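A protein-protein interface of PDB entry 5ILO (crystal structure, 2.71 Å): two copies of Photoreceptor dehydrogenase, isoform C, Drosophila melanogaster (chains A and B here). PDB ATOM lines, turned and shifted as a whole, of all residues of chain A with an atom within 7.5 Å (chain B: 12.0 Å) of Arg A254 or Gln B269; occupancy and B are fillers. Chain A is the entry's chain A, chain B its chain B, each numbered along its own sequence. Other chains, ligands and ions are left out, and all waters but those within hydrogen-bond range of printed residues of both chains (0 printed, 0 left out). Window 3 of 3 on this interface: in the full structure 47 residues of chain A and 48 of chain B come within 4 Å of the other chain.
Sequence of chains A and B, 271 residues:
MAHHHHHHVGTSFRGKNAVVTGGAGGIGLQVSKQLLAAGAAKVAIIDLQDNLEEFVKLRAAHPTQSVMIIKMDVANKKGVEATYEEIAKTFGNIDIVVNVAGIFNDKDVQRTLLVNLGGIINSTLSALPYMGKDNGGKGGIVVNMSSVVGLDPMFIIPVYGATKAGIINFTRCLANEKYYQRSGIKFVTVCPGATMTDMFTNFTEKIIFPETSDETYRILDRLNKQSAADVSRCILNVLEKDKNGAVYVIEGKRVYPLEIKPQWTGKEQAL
No position is printed for both chains.
Of the 9 pairs that touch across the chains among the printed residues, none has its exchanged pair printed and touching as well.
Printed residues of chain A that touch a printed residue of chain B: Val A249, Glu A251, Arg A254, Val A255, Tyr A256 and Pro A257.
Hydrophobic or aromatic side chains of chain A that line the printed part of chain B: Val A249, Tyr A256 and Pro A257.
Among the printed residues, 9 pairs touch across the chains.
Among the printed residues, no Asp or Glu carboxylate lies within 4 Å of a Lys or Arg side-chain nitrogen of the other chain.
Printed residues of chain A within 4 Å of Gln B269: Arg A254 (2.6 Å).
No residue of chain B comes within 4 Å of Cys A234.
Of chain B, only Trp B264 (3.8 Å) comes within 4 Å of Val A249.
No residue of chain B comes within 4 Å of Ile A250.
Gly A252 touches none of the printed residues of chain B.
Val A255 touches one residue of chain B.
Printed residues of chain B within 4 Å of Tyr A256: Trp B264 and Glu B268.
Pro A257 touches just these residues of chain B: Glu B268 and Ala B270.
Of the printed residues of chain B, Glu A251 touches Trp B264 (2.9 Å).
Printed residues of chain A within 4 Å of Ala B270: Arg A254 (3.5 Å), Val A255 (2.9 Å) and Pro A257 (3.9 Å).
Lys A253 touches none of the printed residues of chain B.
Val A231 touches none of the printed residues of chain B.
The indole nitrogen of Trp B264 is in hydrogen-bond range of the side-chain carboxylate of Glu A251 (2.9 Å).
NH2 of Arg A254 lies within hydrogen-bond range of O of Gln B269, at 2.6 Å.
O of Ala B270 sits close to O of Val A255, at 3.1 Å.
The side-chain hydroxyl of Tyr A256 lies close to the guanidinium group of Arg A254 (3.4 Å).
N of Val A249 sits at hydrogen-bond distance from O of Tyr A256, at 2.7 Å.
Val A249 touches Trp B264 (CG1 to CE2, 3.8 Å).
Arg A254 touches Ala B270 (NH2 to CA, 3.5 Å).
CH2 of Trp B264 touches CG of Tyr A256 (3.3 Å).
Glu B268 touches Tyr A256 (CB to CB, 3.4 Å).
O of Pro A257 touches CB of Glu B268 (3.6 Å).
Ala B270 touches Pro A257 (C to CD, 3.9 Å).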
ATOM      1  N   CYS A 191     -19.557   4.673 -11.016  1.00  0.00           N
ATOM      2  CA  CYS A 191     -19.018   3.504 -11.707  1.00  0.00           C
ATOM      3  C   CYS A 191     -19.426   2.202 -11.023  1.00  0.00           C
ATOM      4  O   CYS A 191     -18.715   1.712 -10.145  1.00  0.00           O
ATOM      5  CB  CYS A 191     -17.488   3.580 -11.778  1.00  0.00           C
ATOM      6  SG  CYS A 191     -16.815   5.049 -12.586  1.00  0.00           S
ATOM      7  N   LYS A 225     -24.761  -9.598  -5.427  1.00  0.00           N
ATOM      8  CA  LYS A 225     -24.598  -8.657  -4.313  1.00  0.00           C
ATOM      9  C   LYS A 225     -25.403  -7.359  -4.421  1.00  0.00           C
ATOM     10  O   LYS A 225     -25.865  -6.856  -3.400  1.00  0.00           O
ATOM     11  CB  LYS A 225     -23.123  -8.323  -4.080  1.00  0.00           C
ATOM     12  CG  LYS A 225     -22.405  -9.396  -3.278  1.00  0.00           C
ATOM     13  CD  LYS A 225     -21.093  -8.893  -2.699  1.00  0.00           C
ATOM     14  CE  LYS A 225     -21.114  -8.965  -1.170  1.00  0.00           C
ATOM     15  NZ  LYS A 225     -21.306 -10.359  -0.670  1.00  0.00           N
ATOM     16  N   GLN A 226     -25.556  -6.791  -5.615  1.00  0.00           N
ATOM     17  CA  GLN A 226     -26.384  -5.589  -5.725  1.00  0.00           C
ATOM     18  C   GLN A 226     -27.303  -5.572  -6.949  1.00  0.00           C
ATOM     19  O   GLN A 226     -26.973  -6.097  -8.014  1.00  0.00           O
ATOM     20  CB  GLN A 226     -25.509  -4.328  -5.724  1.00  0.00           C
ATOM     21  CG  GLN A 226     -24.854  -3.998  -7.050  1.00  0.00           C
ATOM     22  CD  GLN A 226     -23.794  -2.926  -6.918  1.00  0.00           C
ATOM     23  OE1 GLN A 226     -23.673  -2.284  -5.874  1.00  0.00           O
ATOM     24  NE2 GLN A 226     -23.020  -2.722  -7.979  1.00  0.00           N
ATOM     25  N   ASP A 230     -30.615  -1.155  -5.571  1.00  0.00           N
ATOM     26  CA  ASP A 230     -29.478  -0.893  -4.687  1.00  0.00           C
ATOM     27  C   ASP A 230     -28.589   0.213  -5.251  1.00  0.00           C
ATOM     28  O   ASP A 230     -28.179   1.121  -4.531  1.00  0.00           O
ATOM     29  CB  ASP A 230     -28.651  -2.164  -4.464  1.00  0.00           C
ATOM     30  CG  ASP A 230     -29.431  -3.253  -3.753  1.00  0.00           C
ATOM     31  OD1 ASP A 230     -30.327  -2.918  -2.952  1.00  0.00           O
ATOM     32  OD2 ASP A 230     -29.144  -4.445  -3.992  1.00  0.00           O
ATOM     33  N   VAL A 231     -28.287   0.118  -6.542  1.00  0.00           N
ATOM     34  CA  VAL A 231     -27.463   1.110  -7.223  1.00  0.00           C
ATOM     35  C   VAL A 231     -28.169   2.464  -7.228  1.00  0.00           C
ATOM     36  O   VAL A 231     -27.550   3.506  -6.998  1.00  0.00           O
ATOM     37  CB  VAL A 231     -27.138   0.682  -8.671  1.00  0.00           C
ATOM     38  CG1 VAL A 231     -26.461   1.811  -9.433  1.00  0.00           C
ATOM     39  CG2 VAL A 231     -26.258  -0.556  -8.671  1.00  0.00           C
ATOM     40  N   CYS A 234     -27.864   4.179  -4.047  1.00  0.00           N
ATOM     41  CA  CYS A 234     -26.516   4.732  -4.037  1.00  0.00           C
ATOM     42  C   CYS A 234     -26.408   6.030  -4.837  1.00  0.00           C
ATOM     43  O   CYS A 234     -25.708   6.955  -4.432  1.00  0.00           O
ATOM     44  CB  CYS A 234     -25.530   3.696  -4.568  1.00  0.00           C
ATOM     45  SG  CYS A 234     -25.245   2.345  -3.412  1.00  0.00           S
ATOM     46  N   ASN A 237     -27.992   8.799  -2.927  1.00  0.00           N
ATOM     47  CA  ASN A 237     -27.007   9.085  -1.888  1.00  0.00           C
ATOM     48  C   ASN A 237     -25.953  10.055  -2.408  1.00  0.00           C
ATOM     49  O   ASN A 237     -25.676  11.086  -1.793  1.00  0.00           O
ATOM     50  CB  ASN A 237     -26.345   7.789  -1.412  1.00  0.00           C
ATOM     51  CG  ASN A 237     -25.452   7.994  -0.198  1.00  0.00           C
ATOM     52  OD1 ASN A 237     -25.307   9.110   0.305  1.00  0.00           O
ATOM     53  ND2 ASN A 237     -24.836   6.915   0.267  1.00  0.00           N
ATOM     54  N   TYR A 248     -17.483   7.945  -8.108  1.00  0.00           N
ATOM     55  CA  TYR A 248     -17.890   6.919  -7.156  1.00  0.00           C
ATOM     56  C   TYR A 248     -17.919   5.533  -7.782  1.00  0.00           C
ATOM     57  O   TYR A 248     -18.315   5.366  -8.933  1.00  0.00           O
ATOM     58  CB  TYR A 248     -19.271   7.247  -6.577  1.00  0.00           C
ATOM     59  CG  TYR A 248     -19.340   8.569  -5.848  1.00  0.00           C
ATOM     60  CD1 TYR A 248     -18.931   8.681  -4.524  1.00  0.00           C
ATOM     61  CD2 TYR A 248     -19.793   9.712  -6.492  1.00  0.00           C
ATOM     62  CE1 TYR A 248     -18.987   9.892  -3.857  1.00  0.00           C
ATOM     63  CE2 TYR A 248     -19.850  10.925  -5.833  1.00  0.00           C
ATOM     64  CZ  TYR A 248     -19.447  11.011  -4.518  1.00  0.00           C
ATOM     65  OH  TYR A 248     -19.508  12.222  -3.870  1.00  0.00           O
ATOM     66  N   VAL A 249     -17.486   4.542  -7.012  1.00  0.00           N
ATOM     67  CA  VAL A 249     -17.689   3.149  -7.375  1.00  0.00           C
ATOM     68  C   VAL A 249     -18.844   2.599  -6.549  1.00  0.00           C
ATOM     69  O   VAL A 249     -18.909   2.818  -5.340  1.00  0.00           O
ATOM     70  CB  VAL A 249     -16.421   2.302  -7.145  1.00  0.00           C
ATOM     71  CG1 VAL A 249     -16.703   0.831  -7.406  1.00  0.00           C
ATOM     72  CG2 VAL A 249     -15.288   2.795  -8.031  1.00  0.00           C
ATOM     73  N   ILE A 250     -19.747   1.874  -7.200  1.00  0.00           N
ATOM     74  CA  ILE A 250     -20.885   1.286  -6.506  1.00  0.00           C
ATOM     75  C   ILE A 250     -20.804  -0.234  -6.577  1.00  0.00           C
ATOM     76  O   ILE A 250     -21.080  -0.838  -7.615  1.00  0.00           O
ATOM     77  CB  ILE A 250     -22.231   1.781  -7.087  1.00  0.00           C
ATOM     78  CG1 ILE A 250     -22.308   3.309  -7.023  1.00  0.00           C
ATOM     79  CG2 ILE A 250     -23.397   1.170  -6.329  1.00  0.00           C
ATOM     80  CD1 ILE A 250     -23.495   3.897  -7.754  1.00  0.00           C
ATOM     81  N   GLU A 251     -20.403  -0.842  -5.464  1.00  0.00           N
ATOM     82  CA  GLU A 251     -20.232  -2.286  -5.391  1.00  0.00           C
ATOM     83  C   GLU A 251     -20.784  -2.846  -4.085  1.00  0.00           C
ATOM     84  O   GLU A 251     -20.532  -2.299  -3.009  1.00  0.00           O
ATOM     85  CB  GLU A 251     -18.752  -2.651  -5.537  1.00  0.00           C
ATOM     86  CG  GLU A 251     -18.491  -4.121  -5.843  1.00  0.00           C
ATOM     87  CD  GLU A 251     -17.367  -4.314  -6.847  1.00  0.00           C
ATOM     88  OE1 GLU A 251     -16.280  -3.731  -6.640  1.00  0.00           O
ATOM     89  OE2 GLU A 251     -17.569  -5.048  -7.841  1.00  0.00           O
ATOM     90  N   GLY A 252     -21.535  -3.939  -4.187  1.00  0.00           N
ATOM     91  CA  GLY A 252     -22.151  -4.561  -3.029  1.00  0.00           C
ATOM     92  C   GLY A 252     -23.075  -3.651  -2.236  1.00  0.00           C
ATOM     93  O   GLY A 252     -22.977  -3.599  -1.007  1.00  0.00           O
ATOM     94  N   LYS A 253     -23.935  -2.909  -2.938  1.00  0.00           N
ATOM     95  CA  LYS A 253     -24.922  -2.011  -2.320  1.00  0.00           C
ATOM     96  C   LYS A 253     -24.275  -0.820  -1.617  1.00  0.00           C
ATOM     97  O   LYS A 253     -24.900  -0.190  -0.763  1.00  0.00           O
ATOM     98  CB  LYS A 253     -25.819  -2.757  -1.316  1.00  0.00           C
ATOM     99  CG  LYS A 253     -26.460  -4.037  -1.828  1.00  0.00           C
ATOM    100  CD  LYS A 253     -27.315  -4.681  -0.742  1.00  0.00           C
ATOM    101  CE  LYS A 253     -27.887  -6.015  -1.199  1.00  0.00           C
ATOM    102  NZ  LYS A 253     -28.621  -6.721  -0.112  1.00  0.00           N
ATOM    103  N   ARG A 254     -23.036  -0.503  -1.977  1.00  0.00           N
ATOM    104  CA  ARG A 254     -22.258   0.462  -1.210  1.00  0.00           C
ATOM    105  C   ARG A 254     -21.523   1.456  -2.111  1.00  0.00           C
ATOM    106  O   ARG A 254     -21.157   1.131  -3.240  1.00  0.00           O
ATOM    107  CB  ARG A 254     -21.271  -0.285  -0.308  1.00  0.00           C
ATOM    108  CG  ARG A 254     -20.526   0.572   0.704  1.00  0.00           C
ATOM    109  CD  ARG A 254     -19.735  -0.304   1.662  1.00  0.00           C
ATOM    110  NE  ARG A 254     -18.780   0.460   2.460  1.00  0.00           N
ATOM    111  CZ  ARG A 254     -17.861  -0.089   3.251  1.00  0.00           C
ATOM    112  NH1 ARG A 254     -17.774  -1.410   3.345  1.00  0.00           N
ATOM    113  NH2 ARG A 254     -17.029   0.677   3.944  1.00  0.00           N
ATOM    114  N   VAL A 255     -21.322   2.672  -1.606  1.00  0.00           N
ATOM    115  CA  VAL A 255     -20.746   3.771  -2.383  1.00  0.00           C
ATOM    116  C   VAL A 255     -19.304   4.055  -1.978  1.00  0.00           C
ATOM    117  O   VAL A 255     -19.036   4.397  -0.828  1.00  0.00           O
ATOM    118  CB  VAL A 255     -21.540   5.079  -2.206  1.00  0.00           C
ATOM    119  CG1 VAL A 255     -20.921   6.186  -3.040  1.00  0.00           C
ATOM    120  CG2 VAL A 255     -22.986   4.884  -2.577  1.00  0.00           C
ATOM    121  N   TYR A 256     -18.377   3.927  -2.918  1.00  0.00           N
ATOM    122  CA  TYR A 256     -16.976   4.217  -2.636  1.00  0.00           C
ATOM    123  C   TYR A 256     -16.436   5.394  -3.453  1.00  0.00           C
ATOM    124  O   TYR A 256     -16.336   5.304  -4.677  1.00  0.00           O
ATOM    125  CB  TYR A 256     -16.115   2.987  -2.907  1.00  0.00           C
ATOM    126  CG  TYR A 256     -16.499   1.740  -2.147  1.00  0.00           C
ATOM    127  CD1 TYR A 256     -15.971   1.483  -0.889  1.00  0.00           C
ATOM    128  CD2 TYR A 256     -17.357   0.802  -2.701  1.00  0.00           C
ATOM    129  CE1 TYR A 256     -16.303   0.335  -0.195  1.00  0.00           C
ATOM    130  CE2 TYR A 256     -17.696  -0.351  -2.016  1.00  0.00           C
ATOM    131  CZ  TYR A 256     -17.164  -0.580  -0.763  1.00  0.00           C
ATOM    132  OH  TYR A 256     -17.496  -1.725  -0.076  1.00  0.00           O
ATOM    133  N   PRO A 257     -16.078   6.498  -2.775  1.00  0.00           N
ATOM    134  CA  PRO A 257     -15.414   7.617  -3.454  1.00  0.00           C
ATOM    135  C   PRO A 257     -13.965   7.281  -3.801  1.00  0.00           C
ATOM    136  O   PRO A 257     -13.255   6.719  -2.966  1.00  0.00           O
ATOM    137  CB  PRO A 257     -15.480   8.747  -2.419  1.00  0.00           C
ATOM    138  CG  PRO A 257     -16.546   8.335  -1.456  1.00  0.00           C
ATOM    139  CD  PRO A 257     -16.455   6.844  -1.397  1.00  0.00           C
ATOM    140  N   GLN B 263      -7.059   1.720 -10.571  1.00  0.00           N
ATOM    141  CA  GLN B 263      -7.815   2.752  -9.870  1.00  0.00           C
ATOM    142  C   GLN B 263      -8.684   2.178  -8.752  1.00  0.00           C
ATOM    143  O   GLN B 263      -8.720   2.721  -7.648  1.00  0.00           O
ATOM    144  CB  GLN B 263      -8.681   3.528 -10.864  1.00  0.00           C
ATOM    145  CG  GLN B 263      -7.870   4.292 -11.898  1.00  0.00           C
ATOM    146  CD  GLN B 263      -7.114   5.458 -11.298  1.00  0.00           C
ATOM    147  OE1 GLN B 263      -7.700   6.325 -10.649  1.00  0.00           O
ATOM    148  NE2 GLN B 263      -5.800   5.479 -11.499  1.00  0.00           N
ATOM    149  N   TRP B 264      -9.386   1.084  -9.037  1.00  0.00           N
ATOM    150  CA  TRP B 264     -10.222   0.452  -8.024  1.00  0.00           C
ATOM    151  C   TRP B 264      -9.532  -0.775  -7.444  1.00  0.00           C
ATOM    152  O   TRP B 264      -9.587  -1.866  -8.016  1.00  0.00           O
ATOM    153  CB  TRP B 264     -11.581   0.081  -8.619  1.00  0.00           C
ATOM    154  CG  TRP B 264     -12.506  -0.603  -7.662  1.00  0.00           C
ATOM    155  CD1 TRP B 264     -13.113  -1.813  -7.833  1.00  0.00           C
ATOM    156  CD2 TRP B 264     -12.920  -0.124  -6.376  1.00  0.00           C
ATOM    157  NE1 TRP B 264     -13.889  -2.111  -6.739  1.00  0.00           N
ATOM    158  CE2 TRP B 264     -13.785  -1.092  -5.830  1.00  0.00           C
ATOM    159  CE3 TRP B 264     -12.647   1.031  -5.637  1.00  0.00           C
ATOM    160  CZ2 TRP B 264     -14.377  -0.940  -4.579  1.00  0.00           C
ATOM    161  CZ3 TRP B 264     -13.236   1.178  -4.398  1.00  0.00           C
ATOM    162  CH2 TRP B 264     -14.090   0.198  -3.880  1.00  0.00           C
ATOM    163  N   THR B 265      -8.922  -0.594  -6.277  1.00  0.00           N
ATOM    164  CA  THR B 265      -8.265  -1.684  -5.565  1.00  0.00           C
ATOM    165  C   THR B 265      -9.011  -2.055  -4.291  1.00  0.00           C
ATOM    166  O   THR B 265      -8.694  -3.056  -3.648  1.00  0.00           O
ATOM    167  CB  THR B 265      -6.808  -1.319  -5.203  1.00  0.00           C
ATOM    168  OG1 THR B 265      -6.799  -0.142  -4.385  1.00  0.00           O
ATOM    169  CG2 THR B 265      -5.994  -1.062  -6.463  1.00  0.00           C
ATOM    170  N   GLY B 266     -10.000  -1.242  -3.925  1.00  0.00           N
ATOM    171  CA  GLY B 266     -10.806  -1.527  -2.753  1.00  0.00           C
ATOM    172  C   GLY B 266     -10.353  -0.739  -1.539  1.00  0.00           C
ATOM    173  O   GLY B 266     -10.886  -0.910  -0.444  1.00  0.00           O
ATOM    174  N   LYS B 267      -9.363   0.129  -1.736  1.00  0.00           N
ATOM    175  CA  LYS B 267      -8.818   0.945  -0.653  1.00  0.00           C
ATOM    176  C   LYS B 267      -9.748   2.085  -0.234  1.00  0.00           C
ATOM    177  O   LYS B 267      -9.458   2.808   0.719  1.00  0.00           O
ATOM    178  CB  LYS B 267      -7.452   1.507  -1.049  1.00  0.00           C
ATOM    179  N   GLU B 268     -10.852   2.246  -0.955  1.00  0.00           N
ATOM    180  CA  GLU B 268     -11.856   3.248  -0.617  1.00  0.00           C
ATOM    181  C   GLU B 268     -12.471   2.887   0.729  1.00  0.00           C
ATOM    182  O   GLU B 268     -12.683   1.710   1.021  1.00  0.00           O
ATOM    183  CB  GLU B 268     -12.927   3.346  -1.697  1.00  0.00           C
ATOM    184  N   GLN B 269     -12.746   3.892   1.554  1.00  0.00           N
ATOM    185  CA  GLN B 269     -13.149   3.638   2.932  1.00  0.00           C
ATOM    186  C   GLN B 269     -14.640   3.318   3.076  1.00  0.00           C
ATOM    187  O   GLN B 269     -14.991   2.302   3.680  1.00  0.00           O
ATOM    188  CB  GLN B 269     -12.793   4.843   3.809  1.00  0.00           C
ATOM    189  N   ALA B 270     -15.511   4.160   2.525  1.00  0.00           N
ATOM    190  CA  ALA B 270     -16.955   3.968   2.684  1.00  0.00           C
ATOM    191  C   ALA B 270     -17.749   4.863   1.742  1.00  0.00           C
ATOM    192  O   ALA B 270     -18.842   5.325   2.078  1.00  0.00           O
ATOM    193  CB  ALA B 270     -17.376   4.224   4.130  1.00  0.00           C
